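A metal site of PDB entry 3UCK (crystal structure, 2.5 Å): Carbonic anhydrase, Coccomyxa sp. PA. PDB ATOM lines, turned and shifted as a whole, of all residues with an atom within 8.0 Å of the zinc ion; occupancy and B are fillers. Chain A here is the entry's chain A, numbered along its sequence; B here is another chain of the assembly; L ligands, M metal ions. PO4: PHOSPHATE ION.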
ATOM      1  N   GLY A  46      24.666   3.212  20.183  1.00  0.00           N
ATOM      2  CA  GLY A  46      25.636   4.085  19.542  1.00  0.00           C
ATOM      3  C   GLY A  46      25.019   4.911  18.448  1.00  0.00           C
ATOM      4  O   GLY A  46      23.810   4.855  18.225  1.00  0.00           O
ATOM      5  N   CYS A  47      25.831   5.632  17.697  1.00  0.00           N
ATOM      6  CA  CYS A  47      25.302   6.599  16.757  1.00  0.00           C
ATOM      7  C   CYS A  47      24.974   5.969  15.434  1.00  0.00           C
ATOM      8  O   CYS A  47      25.621   4.993  14.999  1.00  0.00           O
ATOM      9  CB  CYS A  47      26.284   7.768  16.573  1.00  0.00           C
ATOM     10  SG  CYS A  47      25.617   9.088  15.517  1.00  0.00           S
ATOM     11  N   ALA A  48      23.962   6.518  14.753  1.00  0.00           N
ATOM     12  CA  ALA A  48      23.587   6.023  13.420  1.00  0.00           C
ATOM     13  C   ALA A  48      24.667   6.219  12.340  1.00  0.00           C
ATOM     14  O   ALA A  48      24.555   5.703  11.223  1.00  0.00           O
ATOM     15  CB  ALA A  48      22.301   6.615  12.961  1.00  0.00           C
ATOM     16  N   ASP A  49      25.718   6.961  12.694  1.00  0.00           N
ATOM     17  CA  ASP A  49      26.849   7.262  11.805  1.00  0.00           C
ATOM     18  C   ASP A  49      27.475   6.092  11.040  1.00  0.00           C
ATOM     19  O   ASP A  49      27.889   5.077  11.630  1.00  0.00           O
ATOM     20  CB  ASP A  49      27.939   8.019  12.588  1.00  0.00           C
ATOM     21  CG  ASP A  49      29.046   8.575  11.682  1.00  0.00           C
ATOM     22  OD1 ASP A  49      29.892   7.788  11.263  1.00  0.00           O
ATOM     23  OD2 ASP A  49      29.048   9.777  11.390  1.00  0.00           O
ATOM     24  N   SER A  50      27.632   6.274   9.728  1.00  0.00           N
ATOM     25  CA  SER A  50      28.142   5.227   8.838  1.00  0.00           C
ATOM     26  C   SER A  50      29.549   4.715   9.112  1.00  0.00           C
ATOM     27  O   SER A  50      29.922   3.637   8.560  1.00  0.00           O
ATOM     28  CB  SER A  50      28.070   5.656   7.378  1.00  0.00           C
ATOM     29  OG  SER A  50      28.978   6.723   7.100  1.00  0.00           O
ATOM     30  N   ARG A  51      30.329   5.432   9.930  1.00  0.00           N
ATOM     31  CA  ARG A  51      31.675   4.967  10.228  1.00  0.00           C
ATOM     32  C   ARG A  51      31.725   4.076  11.476  1.00  0.00           C
ATOM     33  O   ARG A  51      32.828   3.689  11.944  1.00  0.00           O
ATOM     34  CB  ARG A  51      32.620   6.142  10.369  1.00  0.00           C
ATOM     35  CG  ARG A  51      32.574   7.032   9.150  1.00  0.00           C
ATOM     36  CD  ARG A  51      33.103   8.395   9.454  1.00  0.00           C
ATOM     37  NE  ARG A  51      32.140   9.280  10.091  1.00  0.00           N
ATOM     38  CZ  ARG A  51      32.452  10.500  10.549  1.00  0.00           C
ATOM     39  NH1 ARG A  51      33.705  10.958  10.443  1.00  0.00           N
ATOM     40  NH2 ARG A  51      31.529  11.240  11.105  1.00  0.00           N
ATOM     41  N   VAL A  52      30.551   3.757  12.040  1.00  0.00           N
ATOM     42  CA  VAL A  52      30.590   3.132  13.373  1.00  0.00           C
ATOM     43  C   VAL A  52      29.741   1.883  13.478  1.00  0.00           C
ATOM     44  O   VAL A  52      28.540   1.916  13.880  1.00  0.00           O
ATOM     45  CB  VAL A  52      30.330   4.141  14.509  1.00  0.00           C
ATOM     46  CG1 VAL A  52      30.697   3.527  15.864  1.00  0.00           C
ATOM     47  CG2 VAL A  52      31.116   5.454  14.253  1.00  0.00           C
ATOM     48  N   ASN A  70      21.043   5.389  16.876  1.00  0.00           N
ATOM     49  CA  ASN A  70      20.299   6.598  16.541  1.00  0.00           C
ATOM     50  C   ASN A  70      21.254   7.771  16.425  1.00  0.00           C
ATOM     51  O   ASN A  70      22.480   7.659  16.778  1.00  0.00           O
ATOM     52  CB  ASN A  70      19.198   6.894  17.574  1.00  0.00           C
ATOM     53  CG  ASN A  70      19.761   7.212  18.955  1.00  0.00           C
ATOM     54  OD1 ASN A  70      20.478   8.217  19.163  1.00  0.00           O
ATOM     55  ND2 ASN A  70      19.436   6.375  19.927  1.00  0.00           N
ATOM     56  N   VAL A  71      20.721   8.865  15.915  1.00  0.00           N
ATOM     57  CA  VAL A  71      21.473  10.114  15.769  1.00  0.00           C
ATOM     58  C   VAL A  71      21.867  10.717  17.119  1.00  0.00           C
ATOM     59  O   VAL A  71      21.043  11.304  17.787  1.00  0.00           O
ATOM     60  CB  VAL A  71      20.681  11.165  14.923  1.00  0.00           C
ATOM     61  CG1 VAL A  71      21.398  12.491  14.944  1.00  0.00           C
ATOM     62  CG2 VAL A  71      20.494  10.676  13.508  1.00  0.00           C
ATOM     63  N   GLY A  72      23.134  10.565  17.513  1.00  0.00           N
ATOM     64  CA  GLY A  72      23.670  11.126  18.744  1.00  0.00           C
ATOM     65  C   GLY A  72      23.801  10.084  19.844  1.00  0.00           C
ATOM     66  O   GLY A  72      24.140  10.425  20.991  1.00  0.00           O
ATOM     67  N   ASN A  73      23.492   8.826  19.540  1.00  0.00           N
ATOM     68  CA  ASN A  73      23.421   7.846  20.597  1.00  0.00           C
ATOM     69  C   ASN A  73      22.736   8.369  21.829  1.00  0.00           C
ATOM     70  O   ASN A  73      23.311   8.391  22.868  1.00  0.00           O
ATOM     71  CB  ASN A  73      24.817   7.271  20.977  1.00  0.00           C
ATOM     72  CG  ASN A  73      25.866   8.333  21.232  1.00  0.00           C
ATOM     73  OD1 ASN A  73      26.613   8.698  20.332  1.00  0.00           O
ATOM     74  ND2 ASN A  73      25.954   8.810  22.475  1.00  0.00           N
ATOM     75  N   CYS A 101      28.035   4.018  23.508  1.00  0.00           N
ATOM     76  CA  CYS A 101      29.139   4.420  22.661  1.00  0.00           C
ATOM     77  C   CYS A 101      28.918   5.694  21.884  1.00  0.00           C
ATOM     78  O   CYS A 101      28.037   5.720  21.035  1.00  0.00           O
ATOM     79  CB  CYS A 101      29.419   3.365  21.614  1.00  0.00           C
ATOM     80  SG  CYS A 101      31.031   3.649  20.772  1.00  0.00           S
ATOM     81  N   GLY A 102      29.755   6.711  22.119  1.00  0.00           N
ATOM     82  CA  GLY A 102      29.725   7.927  21.297  1.00  0.00           C
ATOM     83  C   GLY A 102      30.941   7.896  20.375  1.00  0.00           C
ATOM     84  O   GLY A 102      31.705   6.952  20.393  1.00  0.00           O
ATOM     85  N   HIS A 103      31.110   8.922  19.542  1.00  0.00           N
ATOM     86  CA  HIS A 103      32.219   8.931  18.596  1.00  0.00           C
ATOM     87  C   HIS A 103      32.636  10.357  18.220  1.00  0.00           C
ATOM     88  O   HIS A 103      31.786  11.217  17.874  1.00  0.00           O
ATOM     89  CB  HIS A 103      31.865   8.184  17.322  1.00  0.00           C
ATOM     90  CG  HIS A 103      30.847   8.868  16.502  1.00  0.00           C
ATOM     91  ND1 HIS A 103      31.159   9.769  15.520  1.00  0.00           N
ATOM     92  CD2 HIS A 103      29.492   8.821  16.545  1.00  0.00           C
ATOM     93  CE1 HIS A 103      30.051  10.232  14.974  1.00  0.00           C
ATOM     94  NE2 HIS A 103      29.016   9.668  15.570  1.00  0.00           N
ATOM     95  N   TYR A 104      33.957  10.584  18.235  1.00  0.00           N
ATOM     96  CA  TYR A 104      34.496  11.844  17.726  1.00  0.00           C
ATOM     97  C   TYR A 104      34.005  12.111  16.329  1.00  0.00           C
ATOM     98  O   TYR A 104      33.569  11.209  15.634  1.00  0.00           O
ATOM     99  CB  TYR A 104      36.020  11.879  17.847  1.00  0.00           C
ATOM    100  CG  TYR A 104      36.407  11.801  19.296  1.00  0.00           C
ATOM    101  CD1 TYR A 104      37.100  10.703  19.777  1.00  0.00           C
ATOM    102  CD2 TYR A 104      36.018  12.799  20.204  1.00  0.00           C
ATOM    103  CE1 TYR A 104      37.448  10.600  21.152  1.00  0.00           C
ATOM    104  CE2 TYR A 104      36.356  12.723  21.565  1.00  0.00           C
ATOM    105  CZ  TYR A 104      37.071  11.613  22.029  1.00  0.00           C
ATOM    106  OH  TYR A 104      37.409  11.509  23.362  1.00  0.00           O
ATOM    107  N   ASN A 105      34.032  13.373  15.931  1.00  0.00           N
ATOM    108  CA  ASN A 105      33.471  13.787  14.630  1.00  0.00           C
ATOM    109  C   ASN A 105      31.933  13.629  14.506  1.00  0.00           C
ATOM    110  O   ASN A 105      31.381  13.739  13.402  1.00  0.00           O
ATOM    111  CB  ASN A 105      34.237  13.187  13.431  1.00  0.00           C
ATOM    112  CG  ASN A 105      34.223  14.147  12.197  1.00  0.00           C
ATOM    113  OD1 ASN A 105      33.611  13.875  11.158  1.00  0.00           O
ATOM    114  ND2 ASN A 105      34.863  15.287  12.339  1.00  0.00           N
ATOM    115  N   CYS A 106      31.259  13.405  15.647  1.00  0.00           N
ATOM    116  CA  CYS A 106      29.783  13.244  15.683  1.00  0.00           C
ATOM    117  C   CYS A 106      28.980  14.482  15.333  1.00  0.00           C
ATOM    118  O   CYS A 106      28.852  15.407  16.108  1.00  0.00           O
ATOM    119  CB  CYS A 106      29.265  12.629  17.007  1.00  0.00           C
ATOM    120  SG  CYS A 106      27.386  12.491  16.958  1.00  0.00           S
ATOM    121  N   GLY A 107      28.334  14.439  14.190  1.00  0.00           N
ATOM    122  CA  GLY A 107      27.502  15.536  13.728  1.00  0.00           C
ATOM    123  C   GLY A 107      26.444  16.007  14.681  1.00  0.00           C
ATOM    124  O   GLY A 107      26.068  17.200  14.668  1.00  0.00           O
ATOM    125  N   ALA A 108      25.919  15.082  15.476  1.00  0.00           N
ATOM    126  CA  ALA A 108      24.762  15.392  16.282  1.00  0.00           C
ATOM    127  C   ALA A 108      25.265  16.209  17.436  1.00  0.00           C
ATOM    128  O   ALA A 108      24.648  17.177  17.849  1.00  0.00           O
ATOM    129  CB  ALA A 108      24.139  14.121  16.763  1.00  0.00           C
ATOM    130  N   CYS A 109      26.412  15.821  17.963  1.00  0.00           N
ATOM    131  CA  CYS A 109      27.067  16.638  18.940  1.00  0.00           C
ATOM    132  C   CYS A 109      27.458  18.021  18.409  1.00  0.00           C
ATOM    133  O   CYS A 109      27.242  19.016  19.083  1.00  0.00           O
ATOM    134  CB  CYS A 109      28.261  15.887  19.494  1.00  0.00           C
ATOM    135  SG  CYS A 109      27.662  14.474  20.509  1.00  0.00           S
ATOM    136  N   LYS A 110      27.995  18.106  17.185  1.00  0.00           N
ATOM    137  CA  LYS A 110      28.339  19.438  16.634  1.00  0.00           C
ATOM    138  C   LYS A 110      27.067  20.223  16.493  1.00  0.00           C
ATOM    139  O   LYS A 110      26.974  21.336  17.000  1.00  0.00           O
ATOM    140  CB  LYS A 110      29.103  19.357  15.288  1.00  0.00           C
ATOM    141  CG  LYS A 110      29.565  20.718  14.662  1.00  0.00           C
ATOM    142  CD  LYS A 110      29.141  20.752  13.173  1.00  0.00           C
ATOM    143  CE  LYS A 110      29.911  21.814  12.315  1.00  0.00           C
ATOM    144  NZ  LYS A 110      31.366  21.479  12.015  1.00  0.00           N
ATOM    145  N   TRP A 150      33.814  20.425  20.375  1.00  0.00           N
ATOM    146  CA  TRP A 150      33.257  19.270  19.729  1.00  0.00           C
ATOM    147  C   TRP A 150      33.591  17.977  20.492  1.00  0.00           C
ATOM    148  O   TRP A 150      32.683  17.219  20.869  1.00  0.00           O
ATOM    149  CB  TRP A 150      33.783  19.188  18.332  1.00  0.00           C
ATOM    150  CG  TRP A 150      32.941  18.375  17.428  1.00  0.00           C
ATOM    151  CD1 TRP A 150      31.897  17.536  17.777  1.00  0.00           C
ATOM    152  CD2 TRP A 150      33.081  18.279  16.014  1.00  0.00           C
ATOM    153  NE1 TRP A 150      31.378  16.956  16.651  1.00  0.00           N
ATOM    154  CE2 TRP A 150      32.073  17.387  15.555  1.00  0.00           C
ATOM    155  CE3 TRP A 150      33.950  18.857  15.078  1.00  0.00           C
ATOM    156  CZ2 TRP A 150      31.928  17.072  14.217  1.00  0.00           C
ATOM    157  CZ3 TRP A 150      33.800  18.548  13.734  1.00  0.00           C
ATOM    158  CH2 TRP A 150      32.782  17.663  13.310  1.00  0.00           C
ATOM    159  N   VAL A 154      30.984  15.575  22.757  1.00  0.00           N
ATOM    160  CA  VAL A 154      30.843  14.133  22.480  1.00  0.00           C
ATOM    161  C   VAL A 154      30.993  13.322  23.757  1.00  0.00           C
ATOM    162  O   VAL A 154      30.214  12.402  23.996  1.00  0.00           O
ATOM    163  CB  VAL A 154      31.860  13.640  21.408  1.00  0.00           C
ATOM    164  CG1 VAL A 154      32.058  12.159  21.493  1.00  0.00           C
ATOM    165  CG2 VAL A 154      31.447  14.060  19.995  1.00  0.00           C
ATOM    166  N   ASN A 157      28.167  13.942  26.374  1.00  0.00           N
ATOM    167  CA  ASN A 157      27.031  13.226  25.908  1.00  0.00           C
ATOM    168  C   ASN A 157      27.081  11.745  26.270  1.00  0.00           C
ATOM    169  O   ASN A 157      26.100  11.165  26.724  1.00  0.00           O
ATOM    170  CB  ASN A 157      26.927  13.364  24.419  1.00  0.00           C
ATOM    171  CG  ASN A 157      25.635  12.885  23.929  1.00  0.00           C
ATOM    172  OD1 ASN A 157      24.617  13.092  24.577  1.00  0.00           O
ATOM    173  ND2 ASN A 157      25.641  12.199  22.783  1.00  0.00           N
ATOM    174  N   PRO A 190      36.353   7.810  14.405  1.00  0.00           N
ATOM    175  CA  PRO A 190      36.240   7.415  13.005  1.00  0.00           C
ATOM    176  C   PRO A 190      37.582   7.322  12.259  1.00  0.00           C
ATOM    177  O   PRO A 190      37.767   6.386  11.466  1.00  0.00           O
ATOM    178  CB  PRO A 190      35.293   8.472  12.431  1.00  0.00           C
ATOM    179  CG  PRO A 190      34.364   8.672  13.558  1.00  0.00           C
ATOM    180  CD  PRO A 190      35.242   8.686  14.783  1.00  0.00           C
ATOM    181  N   GLN B  38      31.857  11.779   6.100  1.00  0.00           N
ATOM    182  CA  GLN B  38      31.279  10.542   5.639  1.00  0.00           C
ATOM    183  C   GLN B  38      30.505  10.887   4.385  1.00  0.00           C
ATOM    184  O   GLN B  38      29.884  11.962   4.315  1.00  0.00           O
ATOM    185  CB  GLN B  38      30.332   9.949   6.694  1.00  0.00           C
ATOM    186  CG  GLN B  38      28.956  10.679   6.814  1.00  0.00           C
ATOM    187  CD  GLN B  38      28.246  10.325   8.090  1.00  0.00           C
ATOM    188  OE1 GLN B  38      28.014   9.142   8.411  1.00  0.00           O
ATOM    189  NE2 GLN B  38      27.896  11.340   8.834  1.00  0.00           N
ATOM    190  N   PHE B  66      24.615   4.200   6.578  1.00  0.00           N
ATOM    191  CA  PHE B  66      24.037   4.807   7.764  1.00  0.00           C
ATOM    192  C   PHE B  66      22.947   3.846   8.284  1.00  0.00           C
ATOM    193  O   PHE B  66      22.180   3.277   7.513  1.00  0.00           O
ATOM    194  CB  PHE B  66      23.448   6.157   7.409  1.00  0.00           C
ATOM    195  CG  PHE B  66      23.509   7.187   8.515  1.00  0.00           C
ATOM    196  CD1 PHE B  66      24.660   7.982   8.712  1.00  0.00           C
ATOM    197  CD2 PHE B  66      22.389   7.436   9.310  1.00  0.00           C
ATOM    198  CE1 PHE B  66      24.707   8.950   9.665  1.00  0.00           C
ATOM    199  CE2 PHE B  66      22.424   8.403  10.309  1.00  0.00           C
ATOM    200  CZ  PHE B  66      23.580   9.163  10.484  1.00  0.00           C
ATOM    201  N   TYR B  88      18.232  13.085   8.113  1.00  0.00           N
ATOM    202  CA  TYR B  88      19.618  13.490   8.044  1.00  0.00           C
ATOM    203  C   TYR B  88      20.299  12.809   6.888  1.00  0.00           C
ATOM    204  O   TYR B  88      21.272  13.372   6.337  1.00  0.00           O
ATOM    205  CB  TYR B  88      20.335  13.171   9.330  1.00  0.00           C
ATOM    206  CG  TYR B  88      21.802  13.554   9.367  1.00  0.00           C
ATOM    207  CD1 TYR B  88      22.218  14.893   9.555  1.00  0.00           C
ATOM    208  CD2 TYR B  88      22.791  12.570   9.306  1.00  0.00           C
ATOM    209  CE1 TYR B  88      23.566  15.212   9.633  1.00  0.00           C
ATOM    210  CE2 TYR B  88      24.130  12.877   9.382  1.00  0.00           C
ATOM    211  CZ  TYR B  88      24.524  14.193   9.551  1.00  0.00           C
ATOM    212  OH  TYR B  88      25.878  14.459   9.640  1.00  0.00           O
HETATM  213  P   PO4 L   1      26.520  11.937  12.712  1.00  0.00           P
HETATM  214  O1  PO4 L   1      26.541  10.886  11.625  1.00  0.00           O
HETATM  215  O2  PO4 L   1      26.630  13.294  12.027  1.00  0.00           O
HETATM  216  O3  PO4 L   1      27.688  11.517  13.571  1.00  0.00           O
HETATM  217  O4  PO4 L   1      25.210  11.818  13.461  1.00  0.00           O
HETATM  218 ZN    ZN M   1      27.261  10.712  15.347  1.00  0.00          ZN
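N of Asp 49 lies close to SG of Cys 47 (3.5 Å).
The side-chain sulfur of Cys 47 sits close to the backbone NH of Gly 72 (3.5 Å).
The backbone carbonyl oxygen of Asn 70 sits close to the side-chain sulfur of Cys 47 (3.7 Å).
SG of Cys 106 sits close to N of Ala 108, at 3.3 Å.
The side-chain sulfur (SG) of Cys 106 lies close to the backbone NH (N) of Cys 109 (3.6 Å).
O of Cys 106 lies within hydrogen-bond range of NE1 of Trp 150 (3.0 Å).
The side-chain carboxylate (OD2) of Asp 49 is in salt-bridge range of the guanidinium group (NH2) of Arg 51 (2.9 Å).
The side-chain amide nitrogen of Gln 38 of chain B is in hydrogen-bond range of the side-chain carboxylate of Asp 49 (3.2 Å).
An oxygen (O3) of the ligand is bound to the zinc ion.
NE2 of His 103 is bound to the zinc ion (2.1 Å).
The side-chain sulfur (SG) of Cys 47 is bound to the zinc ion (2.3 Å).
The side-chain sulfur (SG) of Cys 106 is bound to the zinc ion (2.4 Å).
Asp 49 touches the zinc ion (CB to ZN, 3.9 Å).
Within 4 Å of the zinc ion: Cys 47, Asp 49, His 103 and Cys 106.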
